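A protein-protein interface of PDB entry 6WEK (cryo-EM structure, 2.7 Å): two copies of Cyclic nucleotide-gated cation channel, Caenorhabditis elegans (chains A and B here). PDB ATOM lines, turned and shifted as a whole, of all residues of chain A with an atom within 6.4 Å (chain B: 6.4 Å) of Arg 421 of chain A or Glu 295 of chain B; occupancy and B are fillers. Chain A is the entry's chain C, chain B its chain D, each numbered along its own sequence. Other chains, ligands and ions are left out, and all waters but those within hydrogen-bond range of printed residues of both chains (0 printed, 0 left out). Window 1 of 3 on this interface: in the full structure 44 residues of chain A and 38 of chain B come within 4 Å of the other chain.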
ATOM      1  N   SER A 418      19.795  -2.335 -27.653  1.00  0.00           N
ATOM      2  CA  SER A 418      19.989  -1.351 -26.588  1.00  0.00           C
ATOM      3  C   SER A 418      21.270  -0.582 -26.896  1.00  0.00           C
ATOM      4  O   SER A 418      22.349  -0.936 -26.422  1.00  0.00           O
ATOM      5  CB  SER A 418      20.045  -2.027 -25.232  1.00  0.00           C
ATOM      6  OG  SER A 418      18.888  -2.809 -25.013  1.00  0.00           O
ATOM      7  N   ALA A 419      21.147   0.465 -27.705  1.00  0.00           N
ATOM      8  CA  ALA A 419      22.257   1.361 -27.980  1.00  0.00           C
ATOM      9  C   ALA A 419      21.960   2.799 -27.600  1.00  0.00           C
ATOM     10  O   ALA A 419      22.898   3.551 -27.299  1.00  0.00           O
ATOM     11  CB  ALA A 419      22.644   1.306 -29.463  1.00  0.00           C
ATOM     12  N   ALA A 420      20.690   3.200 -27.590  1.00  0.00           N
ATOM     13  CA  ALA A 420      20.329   4.489 -27.020  1.00  0.00           C
ATOM     14  C   ALA A 420      20.641   4.515 -25.534  1.00  0.00           C
ATOM     15  O   ALA A 420      21.223   5.480 -25.027  1.00  0.00           O
ATOM     16  CB  ALA A 420      18.850   4.772 -27.266  1.00  0.00           C
ATOM     17  N   ARG A 421      20.265   3.449 -24.824  1.00  0.00           N
ATOM     18  CA  ARG A 421      20.599   3.343 -23.411  1.00  0.00           C
ATOM     19  C   ARG A 421      22.102   3.373 -23.201  1.00  0.00           C
ATOM     20  O   ARG A 421      22.583   3.960 -22.231  1.00  0.00           O
ATOM     21  CB  ARG A 421      20.010   2.066 -22.820  1.00  0.00           C
ATOM     22  CG  ARG A 421      20.406   1.828 -21.379  1.00  0.00           C
ATOM     23  CD  ARG A 421      19.209   1.892 -20.451  1.00  0.00           C
ATOM     24  NE  ARG A 421      19.601   2.012 -19.052  1.00  0.00           N
ATOM     25  CZ  ARG A 421      19.627   3.159 -18.378  1.00  0.00           C
ATOM     26  NH1 ARG A 421      19.995   3.179 -17.107  1.00  0.00           N
ATOM     27  NH2 ARG A 421      19.281   4.286 -18.975  1.00  0.00           N
ATOM     28  N   THR A 422      22.864   2.768 -24.108  1.00  0.00           N
ATOM     29  CA  THR A 422      24.313   2.745 -23.949  1.00  0.00           C
ATOM     30  C   THR A 422      24.919   4.125 -24.163  1.00  0.00           C
ATOM     31  O   THR A 422      25.823   4.534 -23.428  1.00  0.00           O
ATOM     32  CB  THR A 422      24.922   1.725 -24.905  1.00  0.00           C
ATOM     33  OG1 THR A 422      24.597   0.406 -24.457  1.00  0.00           O
ATOM     34  CG2 THR A 422      26.426   1.875 -24.968  1.00  0.00           C
ATOM     35  N   GLU A 423      24.435   4.865 -25.158  1.00  0.00           N
ATOM     36  CA  GLU A 423      24.916   6.230 -25.346  1.00  0.00           C
ATOM     37  C   GLU A 423      24.568   7.106 -24.146  1.00  0.00           C
ATOM     38  O   GLU A 423      25.400   7.897 -23.670  1.00  0.00           O
ATOM     39  CB  GLU A 423      24.320   6.811 -26.625  1.00  0.00           C
ATOM     40  CG  GLU A 423      24.633   8.269 -26.841  1.00  0.00           C
ATOM     41  CD  GLU A 423      26.041   8.496 -27.337  1.00  0.00           C
ATOM     42  OE1 GLU A 423      26.211   8.702 -28.557  1.00  0.00           O
ATOM     43  OE2 GLU A 423      26.979   8.462 -26.513  1.00  0.00           O
ATOM     44  N   PHE A 424      23.336   6.978 -23.652  1.00  0.00           N
ATOM     45  CA  PHE A 424      22.923   7.698 -22.456  1.00  0.00           C
ATOM     46  C   PHE A 424      23.822   7.361 -21.275  1.00  0.00           C
ATOM     47  O   PHE A 424      24.256   8.253 -20.542  1.00  0.00           O
ATOM     48  CB  PHE A 424      21.468   7.357 -22.147  1.00  0.00           C
ATOM     49  CG  PHE A 424      20.938   7.998 -20.908  1.00  0.00           C
ATOM     50  CD1 PHE A 424      20.364   9.250 -20.957  1.00  0.00           C
ATOM     51  CD2 PHE A 424      20.987   7.339 -19.697  1.00  0.00           C
ATOM     52  CE1 PHE A 424      19.871   9.835 -19.824  1.00  0.00           C
ATOM     53  CE2 PHE A 424      20.499   7.925 -18.562  1.00  0.00           C
ATOM     54  CZ  PHE A 424      19.941   9.170 -18.626  1.00  0.00           C
ATOM     55  N   GLN A 425      23.999   6.105 -21.038  1.00  0.00           N
ATOM     56  CA  GLN A 425      24.900   5.694 -20.007  1.00  0.00           C
ATOM     57  C   GLN A 425      26.466   6.138 -20.136  1.00  0.00           C
ATOM     58  O   GLN A 425      27.342   6.253 -19.318  1.00  0.00           O
ATOM     59  CB  GLN A 425      24.756   4.224 -19.725  1.00  0.00           C
ATOM     60  CG  GLN A 425      23.496   3.824 -18.979  1.00  0.00           C
ATOM     61  CD  GLN A 425      23.234   4.580 -17.673  1.00  0.00           C
ATOM     62  OE1 GLN A 425      22.189   5.158 -17.459  1.00  0.00           O
ATOM     63  NE2 GLN A 425      24.212   4.598 -16.814  1.00  0.00           N
ATOM     64  N   ASN A 426      26.892   6.280 -21.350  1.00  0.00           N
ATOM     65  CA  ASN A 426      28.236   6.816 -21.532  1.00  0.00           C
ATOM     66  C   ASN A 426      28.289   8.291 -21.173  1.00  0.00           C
ATOM     67  O   ASN A 426      29.219   8.738 -20.492  1.00  0.00           O
ATOM     68  CB  ASN A 426      28.707   6.598 -22.966  1.00  0.00           C
ATOM     69  CG  ASN A 426      29.005   5.148 -23.264  1.00  0.00           C
ATOM     70  OD1 ASN A 426      28.480   4.578 -24.216  1.00  0.00           O
ATOM     71  ND2 ASN A 426      29.856   4.542 -22.449  1.00  0.00           N
ATOM     72  N   ASP A 453      18.006  11.637 -14.864  1.00  0.00           N
ATOM     73  CA  ASP A 453      16.994  10.621 -14.600  1.00  0.00           C
ATOM     74  C   ASP A 453      15.663  10.994 -15.242  1.00  0.00           C
ATOM     75  O   ASP A 453      15.042  10.180 -15.936  1.00  0.00           O
ATOM     76  CB  ASP A 453      16.834  10.441 -13.094  1.00  0.00           C
ATOM     77  CG  ASP A 453      16.167   9.140 -12.732  1.00  0.00           C
ATOM     78  OD1 ASP A 453      16.244   8.190 -13.535  1.00  0.00           O
ATOM     79  OD2 ASP A 453      15.565   9.067 -11.642  1.00  0.00           O
ATOM     80  N   TRP A 456      15.641  10.732 -18.899  1.00  0.00           N
ATOM     81  CA  TRP A 456      15.552   9.363 -19.388  1.00  0.00           C
ATOM     82  C   TRP A 456      14.147   8.793 -19.278  1.00  0.00           C
ATOM     83  O   TRP A 456      13.679   8.142 -20.214  1.00  0.00           O
ATOM     84  CB  TRP A 456      16.520   8.454 -18.634  1.00  0.00           C
ATOM     85  CG  TRP A 456      16.413   7.032 -19.069  1.00  0.00           C
ATOM     86  CD1 TRP A 456      15.903   5.995 -18.354  1.00  0.00           C
ATOM     87  CD2 TRP A 456      16.812   6.492 -20.331  1.00  0.00           C
ATOM     88  NE1 TRP A 456      15.967   4.839 -19.088  1.00  0.00           N
ATOM     89  CE2 TRP A 456      16.520   5.121 -20.309  1.00  0.00           C
ATOM     90  CE3 TRP A 456      17.391   7.038 -21.478  1.00  0.00           C
ATOM     91  CZ2 TRP A 456      16.786   4.289 -21.384  1.00  0.00           C
ATOM     92  CZ3 TRP A 456      17.653   6.210 -22.541  1.00  0.00           C
ATOM     93  CH2 TRP A 456      17.353   4.852 -22.488  1.00  0.00           C
ATOM     94  N   VAL B 290      11.441  -4.561 -11.133  1.00  0.00           N
ATOM     95  CA  VAL B 290      12.822  -5.004 -11.007  1.00  0.00           C
ATOM     96  C   VAL B 290      13.703  -4.312 -12.032  1.00  0.00           C
ATOM     97  O   VAL B 290      14.832  -3.917 -11.732  1.00  0.00           O
ATOM     98  CB  VAL B 290      12.890  -6.526 -11.150  1.00  0.00           C
ATOM     99  CG1 VAL B 290      14.308  -6.999 -11.028  1.00  0.00           C
ATOM    100  CG2 VAL B 290      12.034  -7.150 -10.109  1.00  0.00           C
ATOM    101  N   ARG B 291      13.210  -4.162 -13.258  1.00  0.00           N
ATOM    102  CA  ARG B 291      13.997  -3.491 -14.280  1.00  0.00           C
ATOM    103  C   ARG B 291      14.192  -2.025 -13.939  1.00  0.00           C
ATOM    104  O   ARG B 291      15.262  -1.465 -14.186  1.00  0.00           O
ATOM    105  CB  ARG B 291      13.327  -3.644 -15.640  1.00  0.00           C
ATOM    106  CG  ARG B 291      13.837  -2.677 -16.678  1.00  0.00           C
ATOM    107  CD  ARG B 291      13.427  -3.083 -18.077  1.00  0.00           C
ATOM    108  NE  ARG B 291      11.990  -3.298 -18.198  1.00  0.00           N
ATOM    109  CZ  ARG B 291      11.096  -2.323 -18.324  1.00  0.00           C
ATOM    110  NH1 ARG B 291      11.490  -1.058 -18.336  1.00  0.00           N
ATOM    111  NH2 ARG B 291       9.808  -2.613 -18.434  1.00  0.00           N
ATOM    112  N   ASN B 292      13.177  -1.386 -13.363  1.00  0.00           N
ATOM    113  CA  ASN B 292      13.330   0.008 -12.961  1.00  0.00           C
ATOM    114  C   ASN B 292      14.291   0.144 -11.790  1.00  0.00           C
ATOM    115  O   ASN B 292      15.043   1.119 -11.712  1.00  0.00           O
ATOM    116  CB  ASN B 292      11.970   0.605 -12.616  1.00  0.00           C
ATOM    117  CG  ASN B 292      11.044   0.666 -13.813  1.00  0.00           C
ATOM    118  OD1 ASN B 292      11.353   0.142 -14.879  1.00  0.00           O
ATOM    119  ND2 ASN B 292       9.896   1.304 -13.638  1.00  0.00           N
ATOM    120  N   CYS B 293      14.293  -0.827 -10.876  1.00  0.00           N
ATOM    121  CA  CYS B 293      15.221  -0.768  -9.753  1.00  0.00           C
ATOM    122  C   CYS B 293      16.666  -0.801 -10.221  1.00  0.00           C
ATOM    123  O   CYS B 293      17.497  -0.042  -9.724  1.00  0.00           O
ATOM    124  CB  CYS B 293      14.962  -1.913  -8.785  1.00  0.00           C
ATOM    125  SG  CYS B 293      16.214  -2.059  -7.508  1.00  0.00           S
ATOM    126  N   LEU B 294      16.994  -1.671 -11.177  1.00  0.00           N
ATOM    127  CA  LEU B 294      18.376  -1.768 -11.635  1.00  0.00           C
ATOM    128  C   LEU B 294      18.808  -0.526 -12.399  1.00  0.00           C
ATOM    129  O   LEU B 294      19.942  -0.062 -12.241  1.00  0.00           O
ATOM    130  CB  LEU B 294      18.552  -3.007 -12.503  1.00  0.00           C
ATOM    131  CG  LEU B 294      18.146  -4.329 -11.869  1.00  0.00           C
ATOM    132  CD1 LEU B 294      18.447  -5.458 -12.812  1.00  0.00           C
ATOM    133  CD2 LEU B 294      18.864  -4.525 -10.562  1.00  0.00           C
ATOM    134  N   GLU B 295      17.924   0.029 -13.224  1.00  0.00           N
ATOM    135  CA  GLU B 295      18.261   1.249 -13.942  1.00  0.00           C
ATOM    136  C   GLU B 295      18.468   2.412 -12.987  1.00  0.00           C
ATOM    137  O   GLU B 295      19.415   3.190 -13.145  1.00  0.00           O
ATOM    138  CB  GLU B 295      17.172   1.570 -14.956  1.00  0.00           C
ATOM    139  CG  GLU B 295      17.019   0.509 -16.022  1.00  0.00           C
ATOM    140  CD  GLU B 295      15.941   0.844 -17.023  1.00  0.00           C
ATOM    141  OE1 GLU B 295      15.204   1.825 -16.797  1.00  0.00           O
ATOM    142  OE2 GLU B 295      15.830   0.128 -18.039  1.00  0.00           O
ATOM    143  N   ARG B 296      17.610   2.546 -11.977  1.00  0.00           N
ATOM    144  CA  ARG B 296      17.804   3.621 -11.017  1.00  0.00           C
ATOM    145  C   ARG B 296      19.006   3.364 -10.124  1.00  0.00           C
ATOM    146  O   ARG B 296      19.606   4.305  -9.599  1.00  0.00           O
ATOM    147  CB  ARG B 296      16.547   3.818 -10.182  1.00  0.00           C
ATOM    148  CG  ARG B 296      15.663   4.910 -10.724  1.00  0.00           C
ATOM    149  CD  ARG B 296      14.599   5.268  -9.732  1.00  0.00           C
ATOM    150  NE  ARG B 296      13.773   4.112  -9.432  1.00  0.00           N
ATOM    151  CZ  ARG B 296      12.750   4.128  -8.592  1.00  0.00           C
ATOM    152  NH1 ARG B 296      12.423   5.246  -7.960  1.00  0.00           N
ATOM    153  NH2 ARG B 296      12.055   3.022  -8.388  1.00  0.00           N
ATOM    154  N   THR B 297      19.367   2.101  -9.920  1.00  0.00           N
ATOM    155  CA  THR B 297      20.546   1.805  -9.121  1.00  0.00           C
ATOM    156  C   THR B 297      21.816   2.186  -9.857  1.00  0.00           C
ATOM    157  O   THR B 297      22.761   2.688  -9.246  1.00  0.00           O
ATOM    158  CB  THR B 297      20.575   0.331  -8.748  1.00  0.00           C
ATOM    159  OG1 THR B 297      19.334  -0.028  -8.142  1.00  0.00           O
ATOM    160  CG2 THR B 297      21.686   0.067  -7.767  1.00  0.00           C
ATOM    161  N   GLU B 298      21.868   1.940 -11.163  1.00  0.00           N
ATOM    162  CA  GLU B 298      23.068   2.330 -11.893  1.00  0.00           C
ATOM    163  C   GLU B 298      23.076   3.817 -12.207  1.00  0.00           C
ATOM    164  O   GLU B 298      24.146   4.389 -12.430  1.00  0.00           O
ATOM    165  CB  GLU B 298      23.224   1.509 -13.165  1.00  0.00           C
ATOM    166  CG  GLU B 298      22.318   1.900 -14.289  1.00  0.00           C
ATOM    167  CD  GLU B 298      22.669   1.180 -15.563  1.00  0.00           C
ATOM    168  OE1 GLU B 298      23.864   0.886 -15.758  1.00  0.00           O
ATOM    169  OE2 GLU B 298      21.758   0.899 -16.368  1.00  0.00           O
ATOM    170  N   THR B 299      21.912   4.463 -12.226  1.00  0.00           N
ATOM    171  CA  THR B 299      21.887   5.914 -12.356  1.00  0.00           C
ATOM    172  C   THR B 299      22.306   6.622 -11.074  1.00  0.00           C
ATOM    173  O   THR B 299      22.765   7.764 -11.136  1.00  0.00           O
ATOM    174  CB  THR B 299      20.494   6.373 -12.779  1.00  0.00           C
ATOM    175  OG1 THR B 299      20.084   5.628 -13.929  1.00  0.00           O
ATOM    176  CG2 THR B 299      20.494   7.834 -13.138  1.00  0.00           C
ATOM    177  N   ARG B 300      22.189   5.971  -9.922  1.00  0.00           N
ATOM    178  CA  ARG B 300      22.584   6.550  -8.649  1.00  0.00           C
ATOM    179  C   ARG B 300      23.953   6.090  -8.194  1.00  0.00           C
ATOM    180  O   ARG B 300      24.464   6.600  -7.197  1.00  0.00           O
ATOM    181  CB  ARG B 300      21.572   6.188  -7.558  1.00  0.00           C
ATOM    182  CG  ARG B 300      20.211   6.799  -7.699  1.00  0.00           C
ATOM    183  CD  ARG B 300      19.213   5.991  -6.907  1.00  0.00           C
ATOM    184  NE  ARG B 300      18.476   6.789  -5.937  1.00  0.00           N
ATOM    185  CZ  ARG B 300      18.786   6.871  -4.651  1.00  0.00           C
ATOM    186  NH1 ARG B 300      19.829   6.209  -4.170  1.00  0.00           N
ATOM    187  NH2 ARG B 300      18.054   7.618  -3.842  1.00  0.00           N
ATOM    188  N   PHE B 307      28.774  -1.977 -10.959  1.00  0.00           N
ATOM    189  CA  PHE B 307      27.408  -2.450 -10.786  1.00  0.00           C
ATOM    190  C   PHE B 307      26.928  -3.194 -12.021  1.00  0.00           C
ATOM    191  O   PHE B 307      26.248  -4.215 -11.911  1.00  0.00           O
ATOM    192  CB  PHE B 307      26.479  -1.284 -10.468  1.00  0.00           C
ATOM    193  CG  PHE B 307      25.046  -1.683 -10.363  1.00  0.00           C
ATOM    194  CD1 PHE B 307      24.594  -2.392  -9.271  1.00  0.00           C
ATOM    195  CD2 PHE B 307      24.152  -1.367 -11.363  1.00  0.00           C
ATOM    196  CE1 PHE B 307      23.289  -2.772  -9.179  1.00  0.00           C
ATOM    197  CE2 PHE B 307      22.844  -1.747 -11.273  1.00  0.00           C
ATOM    198  CZ  PHE B 307      22.413  -2.448 -10.178  1.00  0.00           C
ATOM    199  N   ARG B 308      27.260  -2.692 -13.208  1.00  0.00           N
ATOM    200  CA  ARG B 308      26.869  -3.389 -14.426  1.00  0.00           C
ATOM    201  C   ARG B 308      27.497  -4.770 -14.496  1.00  0.00           C
ATOM    202  O   ARG B 308      26.843  -5.739 -14.895  1.00  0.00           O
ATOM    203  CB  ARG B 308      27.255  -2.567 -15.647  1.00  0.00           C
ATOM    204  CG  ARG B 308      26.434  -1.329 -15.820  1.00  0.00           C
ATOM    205  CD  ARG B 308      26.593  -0.769 -17.204  1.00  0.00           C
ATOM    206  NE  ARG B 308      27.532   0.339 -17.246  1.00  0.00           N
ATOM    207  CZ  ARG B 308      27.197   1.598 -17.004  1.00  0.00           C
ATOM    208  NH1 ARG B 308      25.949   1.901 -16.698  1.00  0.00           N
ATOM    209  NH2 ARG B 308      28.107   2.552 -17.063  1.00  0.00           N
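Among the printed residues, pairs that only touch across the chains: Trp 456 of chain A with Glu 295 of chain B (3.9 Å), Gln 425 of chain A with Glu 298 of chain B (3.9 Å) and Arg 421 of chain A with Glu 295 of chain B (3.9 Å).
Of the printed residues of chain B, Arg 421 of chain A touches Glu 295 and Glu 298.
Of the printed residues of chain B, Gln 425 of chain A touches Glu 298 and Arg 308.
Printed residues of chain B within 4 Å of Trp 456 of chain A: Glu 295.
Glu 295 of chain B touches just these residues of chain A: Arg 421 and Trp 456.
Of the printed residues of chain A, Glu 298 of chain B touches Arg 421 and Gln 425.
Of the printed residues of chain A, Arg 308 of chain B touches Gln 425 (3.2 Å).
NH1 of Arg 421 of chain A is in salt-bridge range of OE2 of Glu 298 of chain B (3.0 Å).
NE2 of Gln 425 of chain A lies close to NH1 of Arg 308 of chain B, 3.2 Å away.
No position is printed for both chains.
OE1 of Gln 425 of chain A lies within hydrogen-bond range of NH1 of Arg 421 of chain A, at 3.0 Å.
The backbone carbonyl oxygen (O) of Glu 295 of chain B lies within hydrogen-bond range of the side-chain hydroxyl (OG1) of Thr 299 of chain B (2.6 Å).
The side-chain carboxylate of Glu 298 of chain B lies within salt-bridge range of the guanidinium group of Arg 308 of chain B (2.5 Å).
Among the printed residues, Asp or Glu carboxylates within 4 Å of a Lys or Arg side-chain nitrogen of the other chain: Arg 421 of chain A with Glu 298 of chain B (3.0 Å).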
